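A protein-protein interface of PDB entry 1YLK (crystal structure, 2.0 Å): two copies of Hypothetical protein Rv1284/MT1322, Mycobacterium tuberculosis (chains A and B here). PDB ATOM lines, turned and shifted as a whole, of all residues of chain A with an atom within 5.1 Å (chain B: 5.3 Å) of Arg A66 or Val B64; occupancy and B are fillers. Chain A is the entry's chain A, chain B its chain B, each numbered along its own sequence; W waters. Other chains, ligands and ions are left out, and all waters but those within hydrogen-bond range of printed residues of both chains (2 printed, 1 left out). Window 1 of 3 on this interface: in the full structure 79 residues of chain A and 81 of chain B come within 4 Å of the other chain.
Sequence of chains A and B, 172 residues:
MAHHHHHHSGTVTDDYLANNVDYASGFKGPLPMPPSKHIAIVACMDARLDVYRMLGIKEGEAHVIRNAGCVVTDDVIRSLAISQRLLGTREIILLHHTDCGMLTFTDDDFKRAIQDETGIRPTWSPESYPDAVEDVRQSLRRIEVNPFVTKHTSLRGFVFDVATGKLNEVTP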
ATOM      1  N   ALA A  43     -26.711  -5.928  20.356  1.00  0.00           N
ATOM      2  CA  ALA A  43     -25.960  -5.426  21.488  1.00  0.00           C
ATOM      3  C   ALA A  43     -25.436  -4.022  21.199  1.00  0.00           C
ATOM      4  O   ALA A  43     -25.434  -3.587  20.042  1.00  0.00           O
ATOM      5  CB  ALA A  43     -24.809  -6.380  21.822  1.00  0.00           C
ATOM      6  N   CYS A  44     -25.024  -3.299  22.247  1.00  0.00           N
ATOM      7  CA  CYS A  44     -24.352  -2.007  22.030  1.00  0.00           C
ATOM      8  C   CYS A  44     -22.964  -2.282  21.485  1.00  0.00           C
ATOM      9  O   CYS A  44     -22.389  -3.329  21.776  1.00  0.00           O
ATOM     10  CB  CYS A  44     -24.194  -1.223  23.337  1.00  0.00           C
ATOM     11  SG  CYS A  44     -23.472   0.438  23.105  1.00  0.00           S
ATOM     12  N   MET A  45     -22.416  -1.311  20.760  1.00  0.00           N
ATOM     13  CA  MET A  45     -21.050  -1.372  20.242  1.00  0.00           C
ATOM     14  C   MET A  45     -19.999  -1.153  21.339  1.00  0.00           C
ATOM     15  O   MET A  45     -18.812  -1.297  21.080  1.00  0.00           O
ATOM     16  CB  MET A  45     -20.853  -0.302  19.175  1.00  0.00           C
ATOM     17  CG  MET A  45     -20.779   1.121  19.728  1.00  0.00           C
ATOM     18  SD  MET A  45     -20.611   2.324  18.413  1.00  0.00           S
ATOM     19  CE  MET A  45     -20.517   3.893  19.277  1.00  0.00           C
ATOM     20  N   ASP A  46     -20.451  -0.812  22.543  1.00  0.00           N
ATOM     21  CA  ASP A  46     -19.582  -0.504  23.682  1.00  0.00           C
ATOM     22  C   ASP A  46     -18.334  -1.399  23.782  1.00  0.00           C
ATOM     23  O   ASP A  46     -18.413  -2.639  23.695  1.00  0.00           O
ATOM     24  CB  ASP A  46     -20.384  -0.539  24.996  1.00  0.00           C
ATOM     25  CG  ASP A  46     -19.640   0.108  26.156  1.00  0.00           C
ATOM     26  OD1 ASP A  46     -18.733  -0.530  26.706  1.00  0.00           O
ATOM     27  OD2 ASP A  46     -19.955   1.253  26.527  1.00  0.00           O
ATOM     28  N   LEU A  49     -18.042  -4.555  26.170  1.00  0.00           N
ATOM     29  CA  LEU A  49     -18.874  -5.727  25.929  1.00  0.00           C
ATOM     30  C   LEU A  49     -18.236  -6.663  24.920  1.00  0.00           C
ATOM     31  O   LEU A  49     -18.237  -6.398  23.725  1.00  0.00           O
ATOM     32  CB  LEU A  49     -20.270  -5.306  25.449  1.00  0.00           C
ATOM     33  CG  LEU A  49     -21.314  -4.898  26.489  1.00  0.00           C
ATOM     34  CD1 LEU A  49     -20.899  -3.667  27.266  1.00  0.00           C
ATOM     35  CD2 LEU A  49     -22.643  -4.660  25.760  1.00  0.00           C
ATOM     36  N   ASP A  50     -17.676  -7.756  25.424  1.00  0.00           N
ATOM     37  CA  ASP A  50     -17.225  -8.863  24.591  1.00  0.00           C
ATOM     38  C   ASP A  50     -18.393  -9.847  24.558  1.00  0.00           C
ATOM     39  O   ASP A  50     -18.506 -10.707  25.429  1.00  0.00           O
ATOM     40  CB  ASP A  50     -15.958  -9.486  25.204  1.00  0.00           C
ATOM     41  CG  ASP A  50     -15.441 -10.708  24.429  1.00  0.00           C
ATOM     42  OD1 ASP A  50     -16.101 -11.203  23.501  1.00  0.00           O
ATOM     43  OD2 ASP A  50     -14.348 -11.185  24.779  1.00  0.00           O
ATOM     44  N   VAL A  51     -19.255  -9.701  23.549  1.00  0.00           N
ATOM     45  CA  VAL A  51     -20.551 -10.396  23.498  1.00  0.00           C
ATOM     46  C   VAL A  51     -20.406 -11.922  23.472  1.00  0.00           C
ATOM     47  O   VAL A  51     -21.148 -12.643  24.139  1.00  0.00           O
ATOM     48  CB  VAL A  51     -21.405  -9.874  22.310  1.00  0.00           C
ATOM     49  CG1 VAL A  51     -22.677 -10.711  22.135  1.00  0.00           C
ATOM     50  CG2 VAL A  51     -21.755  -8.403  22.531  1.00  0.00           C
ATOM     51  N   VAL A  64     -24.441 -11.677  15.546  1.00  0.00           N
ATOM     52  CA  VAL A  64     -24.305 -10.618  16.523  1.00  0.00           C
ATOM     53  C   VAL A  64     -24.424  -9.296  15.785  1.00  0.00           C
ATOM     54  O   VAL A  64     -23.675  -9.024  14.842  1.00  0.00           O
ATOM     55  CB  VAL A  64     -22.985 -10.718  17.352  1.00  0.00           C
ATOM     56  CG1 VAL A  64     -22.807  -9.499  18.217  1.00  0.00           C
ATOM     57  CG2 VAL A  64     -22.979 -12.005  18.222  1.00  0.00           C
ATOM     58  N   ILE A  65     -25.402  -8.504  16.202  1.00  0.00           N
ATOM     59  CA  ILE A  65     -25.700  -7.227  15.596  1.00  0.00           C
ATOM     60  C   ILE A  65     -25.379  -6.188  16.663  1.00  0.00           C
ATOM     61  O   ILE A  65     -25.766  -6.344  17.828  1.00  0.00           O
ATOM     62  CB  ILE A  65     -27.190  -7.133  15.166  1.00  0.00           C
ATOM     63  CG1 ILE A  65     -27.505  -8.206  14.103  1.00  0.00           C
ATOM     64  CG2 ILE A  65     -27.533  -5.717  14.649  1.00  0.00           C
ATOM     65  CD1 ILE A  65     -28.994  -8.566  13.934  1.00  0.00           C
ATOM     66  N   ARG A  66     -24.650  -5.146  16.274  1.00  0.00           N
ATOM     67  CA  ARG A  66     -24.219  -4.142  17.239  1.00  0.00           C
ATOM     68  C   ARG A  66     -24.234  -2.747  16.663  1.00  0.00           C
ATOM     69  O   ARG A  66     -23.821  -2.524  15.510  1.00  0.00           O
ATOM     70  CB  ARG A  66     -22.806  -4.457  17.748  1.00  0.00           C
ATOM     71  CG  ARG A  66     -22.648  -5.848  18.314  1.00  0.00           C
ATOM     72  CD  ARG A  66     -21.226  -6.051  18.871  1.00  0.00           C
ATOM     73  NE  ARG A  66     -21.012  -5.278  20.086  1.00  0.00           N
ATOM     74  CZ  ARG A  66     -19.992  -5.462  20.926  1.00  0.00           C
ATOM     75  NH1 ARG A  66     -19.104  -6.423  20.699  1.00  0.00           N
ATOM     76  NH2 ARG A  66     -19.884  -4.703  22.010  1.00  0.00           N
ATOM     77  N   ASN A  67     -24.719  -1.802  17.471  1.00  0.00           N
ATOM     78  CA  ASN A  67     -24.657  -0.387  17.098  1.00  0.00           C
ATOM     79  C   ASN A  67     -24.564   0.503  18.341  1.00  0.00           C
ATOM     80  O   ASN A  67     -24.563   0.003  19.467  1.00  0.00           O
ATOM     81  CB  ASN A  67     -25.846  -0.018  16.188  1.00  0.00           C
ATOM     82  CG  ASN A  67     -27.204  -0.089  16.905  1.00  0.00           C
ATOM     83  OD1 ASN A  67     -27.283  -0.095  18.123  1.00  0.00           O
ATOM     84  ND2 ASN A  67     -28.280  -0.124  16.125  1.00  0.00           N
ATOM     85  N   ALA A  68     -24.515   1.811  18.157  1.00  0.00           N
ATOM     86  CA  ALA A  68     -24.485   2.708  19.311  1.00  0.00           C
ATOM     87  C   ALA A  68     -25.808   2.638  20.091  1.00  0.00           C
ATOM     88  O   ALA A  68     -26.858   2.983  19.560  1.00  0.00           O
ATOM     89  CB  ALA A  68     -24.201   4.152  18.857  1.00  0.00           C
ATOM     90  N   ILE B  41     -14.596  -0.813  14.807  1.00  0.00           N
ATOM     91  CA  ILE B  41     -14.624  -1.893  13.825  1.00  0.00           C
ATOM     92  C   ILE B  41     -16.056  -2.005  13.363  1.00  0.00           C
ATOM     93  O   ILE B  41     -16.982  -2.024  14.178  1.00  0.00           O
ATOM     94  CB  ILE B  41     -14.250  -3.292  14.430  1.00  0.00           C
ATOM     95  CG1 ILE B  41     -13.006  -3.264  15.343  1.00  0.00           C
ATOM     96  CG2 ILE B  41     -14.161  -4.363  13.328  1.00  0.00           C
ATOM     97  CD1 ILE B  41     -11.769  -2.677  14.763  1.00  0.00           C
ATOM     98  N   ALA B  43     -18.256  -4.678  11.133  1.00  0.00           N
ATOM     99  CA  ALA B  43     -18.172  -6.040  10.593  1.00  0.00           C
ATOM    100  C   ALA B  43     -19.547  -6.599  10.225  1.00  0.00           C
ATOM    101  O   ALA B  43     -20.573  -6.019  10.584  1.00  0.00           O
ATOM    102  CB  ALA B  43     -17.481  -6.966  11.597  1.00  0.00           C
ATOM    103  N   VAL B  51     -15.133 -11.334  16.008  1.00  0.00           N
ATOM    104  CA  VAL B  51     -14.312 -10.148  15.736  1.00  0.00           C
ATOM    105  C   VAL B  51     -13.185  -9.975  16.764  1.00  0.00           C
ATOM    106  O   VAL B  51     -12.023  -9.716  16.392  1.00  0.00           O
ATOM    107  CB  VAL B  51     -15.208  -8.869  15.623  1.00  0.00           C
ATOM    108  CG1 VAL B  51     -14.349  -7.606  15.439  1.00  0.00           C
ATOM    109  CG2 VAL B  51     -16.188  -9.028  14.451  1.00  0.00           C
ATOM    110  N   TYR B  52     -13.515 -10.154  18.052  1.00  0.00           N
ATOM    111  CA  TYR B  52     -12.518 -10.023  19.127  1.00  0.00           C
ATOM    112  C   TYR B  52     -11.346 -10.984  18.953  1.00  0.00           C
ATOM    113  O   TYR B  52     -10.179 -10.594  19.088  1.00  0.00           O
ATOM    114  CB  TYR B  52     -13.161 -10.220  20.510  1.00  0.00           C
ATOM    115  CG  TYR B  52     -13.715  -8.961  21.160  1.00  0.00           C
ATOM    116  CD1 TYR B  52     -14.721  -8.208  20.545  1.00  0.00           C
ATOM    117  CD2 TYR B  52     -13.266  -8.552  22.417  1.00  0.00           C
ATOM    118  CE1 TYR B  52     -15.215  -7.046  21.143  1.00  0.00           C
ATOM    119  CE2 TYR B  52     -13.776  -7.412  23.031  1.00  0.00           C
ATOM    120  CZ  TYR B  52     -14.744  -6.669  22.391  1.00  0.00           C
ATOM    121  OH  TYR B  52     -15.242  -5.535  23.014  1.00  0.00           O
ATOM    122  N   ILE B  57      -8.543  -8.527  20.035  1.00  0.00           N
ATOM    123  CA  ILE B  57      -9.110  -7.407  20.795  1.00  0.00           C
ATOM    124  C   ILE B  57      -9.314  -7.823  22.252  1.00  0.00           C
ATOM    125  O   ILE B  57      -9.761  -8.934  22.525  1.00  0.00           O
ATOM    126  CB  ILE B  57     -10.462  -6.948  20.176  1.00  0.00           C
ATOM    127  CG1 ILE B  57     -10.282  -6.515  18.715  1.00  0.00           C
ATOM    128  CG2 ILE B  57     -11.086  -5.806  20.975  1.00  0.00           C
ATOM    129  CD1 ILE B  57     -11.606  -6.271  17.968  1.00  0.00           C
ATOM    130  N   ALA B  62     -12.010  -1.370  21.928  1.00  0.00           N
ATOM    131  CA  ALA B  62     -12.555  -1.101  20.592  1.00  0.00           C
ATOM    132  C   ALA B  62     -14.071  -1.142  20.540  1.00  0.00           C
ATOM    133  O   ALA B  62     -14.680  -2.049  21.090  1.00  0.00           O
ATOM    134  CB  ALA B  62     -12.010  -2.131  19.575  1.00  0.00           C
ATOM    135  N   HIS B  63     -14.664  -0.189  19.822  1.00  0.00           N
ATOM    136  CA  HIS B  63     -16.051  -0.305  19.419  1.00  0.00           C
ATOM    137  C   HIS B  63     -16.194  -1.324  18.306  1.00  0.00           C
ATOM    138  O   HIS B  63     -15.402  -1.337  17.348  1.00  0.00           O
ATOM    139  CB  HIS B  63     -16.601   1.034  18.957  1.00  0.00           C
ATOM    140  CG  HIS B  63     -16.897   1.976  20.074  1.00  0.00           C
ATOM    141  ND1 HIS B  63     -16.735   3.338  19.956  1.00  0.00           N
ATOM    142  CD2 HIS B  63     -17.350   1.756  21.331  1.00  0.00           C
ATOM    143  CE1 HIS B  63     -17.092   3.917  21.084  1.00  0.00           C
ATOM    144  NE2 HIS B  63     -17.456   2.978  21.938  1.00  0.00           N
ATOM    145  N   VAL B  64     -17.215  -2.169  18.419  1.00  0.00           N
ATOM    146  CA  VAL B  64     -17.519  -3.094  17.349  1.00  0.00           C
ATOM    147  C   VAL B  64     -18.974  -2.882  16.908  1.00  0.00           C
ATOM    148  O   VAL B  64     -19.910  -3.009  17.717  1.00  0.00           O
ATOM    149  CB  VAL B  64     -17.228  -4.578  17.748  1.00  0.00           C
ATOM    150  CG1 VAL B  64     -17.726  -5.536  16.669  1.00  0.00           C
ATOM    151  CG2 VAL B  64     -15.721  -4.785  18.003  1.00  0.00           C
ATOM    152  N   ILE B  65     -19.142  -2.542  15.635  1.00  0.00           N
ATOM    153  CA  ILE B  65     -20.458  -2.282  15.028  1.00  0.00           C
ATOM    154  C   ILE B  65     -20.673  -3.413  14.024  1.00  0.00           C
ATOM    155  O   ILE B  65     -19.762  -3.724  13.234  1.00  0.00           O
ATOM    156  CB  ILE B  65     -20.484  -0.898  14.296  1.00  0.00           C
ATOM    157  CG1 ILE B  65     -20.176   0.228  15.287  1.00  0.00           C
ATOM    158  CG2 ILE B  65     -21.850  -0.650  13.574  1.00  0.00           C
ATOM    159  CD1 ILE B  65     -19.520   1.514  14.705  1.00  0.00           C
ATOM    160  N   ARG B  66     -21.857  -4.015  14.042  1.00  0.00           N
ATOM    161  CA  ARG B  66     -22.141  -5.171  13.194  1.00  0.00           C
ATOM    162  C   ARG B  66     -23.558  -5.094  12.648  1.00  0.00           C
ATOM    163  O   ARG B  66     -24.515  -4.752  13.366  1.00  0.00           O
ATOM    164  CB  ARG B  66     -21.923  -6.489  13.948  1.00  0.00           C
ATOM    165  CG  ARG B  66     -20.539  -6.631  14.605  1.00  0.00           C
ATOM    166  CD  ARG B  66     -20.336  -7.982  15.261  1.00  0.00           C
ATOM    167  NE  ARG B  66     -20.214  -9.056  14.279  1.00  0.00           N
ATOM    168  CZ  ARG B  66     -19.772 -10.281  14.550  1.00  0.00           C
ATOM    169  NH1 ARG B  66     -19.330 -10.598  15.766  1.00  0.00           N
ATOM    170  NH2 ARG B  66     -19.736 -11.181  13.585  1.00  0.00           N
ATOM    171  N   ASN B  67     -23.692  -5.390  11.364  1.00  0.00           N
ATOM    172  CA  ASN B  67     -25.019  -5.551  10.781  1.00  0.00           C
ATOM    173  C   ASN B  67     -24.954  -6.571   9.671  1.00  0.00           C
ATOM    174  O   ASN B  67     -23.875  -7.110   9.410  1.00  0.00           O
ATOM    175  CB  ASN B  67     -25.583  -4.192  10.325  1.00  0.00           C
ATOM    176  CG  ASN B  67     -24.783  -3.573   9.188  1.00  0.00           C
ATOM    177  OD1 ASN B  67     -24.037  -4.258   8.487  1.00  0.00           O
ATOM    178  ND2 ASN B  67     -24.939  -2.258   9.003  1.00  0.00           N
HETATM  179  O   HOH W   1     -17.498   2.212  24.689  1.00  0.00           O
HETATM  180  O   HOH W   2     -18.847  -8.891  18.547  1.00  0.00           O
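Water W1 bridges a ring nitrogen (NE2) of His B63 (2.9 Å) and the side-chain carboxylate (OD2) of Asp A46 (3.2 Å). Water W2 bridges the guanidinium group (NH1) of Arg A66 (3.3 Å) and the guanidinium group (NH1) of Arg B66 (3.3 Å).
Val A64 touches Arg B66, and with the chains exchanged Arg A66 touches Val B64. Ile A65 touches Arg B66, and with the chains exchanged Arg A66 touches Ile B65. Arg B66 touches its own counterpart, Arg A66.
Of chain B, only Tyr B52, Val B64, Ile B65 and Arg B66 come within 4 Å of Arg A66. Printed residues of chain A within 4 Å of Tyr B52: Leu A49 (3.2 Å), Asp A50 (3.7 Å) and Arg A66 (3.96 Å). Of the printed residues of chain B, Asp A50 touches Tyr B52 (3.7 Å). Val A51 touches none of the printed residues of chain B. Asn B67 touches none of the printed residues of chain A. The nearest residue of chain A that does not touch Val B64 is Cys A44 (4.8 Å). The nearest printed residue of chain B that does not touch Met A45 is Ala B62 (4.2 Å).
Hydrophobic or aromatic side chains of chain A within 4 Å of the printed part of chain B: Met A45, Val A64 and Ile A65. Among the printed residues, 12 pairs touch across the chains. Among the printed residues, no Asp or Glu carboxylate lies within 4 Å of a Lys or Arg side-chain nitrogen of the other chain.
The backbone carbonyl oxygen of Met A45 is in hydrogen-bond range of the backbone NH of Val B64, 3.2 Å away. O of Leu A49 sits at hydrogen-bond distance from OH of Tyr B52 (3.2 Å). NE of Arg A66 lies close to O of Val B64 (3.5 Å). O of Arg A66 is in hydrogen-bond range of N of Arg B66.
The backbone carbonyl oxygen (O) of Cys A44 lies within hydrogen-bond range of the guanidinium group (NH2) of Arg A66. The backbone carbonyl oxygen (O) of Asp A46 sits at hydrogen-bond distance from the guanidinium group (NH2) of Arg A66, at 3.0 Å. The backbone NH of Ile B41 lies within hydrogen-bond range of the backbone carbonyl oxygen of His B63 (2.7 Å). The backbone NH (N) of Ile B65 lies within hydrogen-bond range of the backbone carbonyl oxygen (O) of Ile B41, at 2.7 Å. O of Ile B65 lies within hydrogen-bond range of N of Ala B43, 2.8 Å away. The backbone NH (N) of Ile B57 lies within hydrogen-bond range of the backbone carbonyl oxygen (O) of Tyr B52 (2.8 Å).
Among the printed residues, merely in contact across the chains: Met A45 with His B63, Met A45 with Ile B65, Asp A46 with His B63, Asp A50 with Tyr B52, Val A64 with Arg B66, Ile A65 with Arg B66, Arg A66 with Tyr B52 and Arg A66 with Ile B65.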
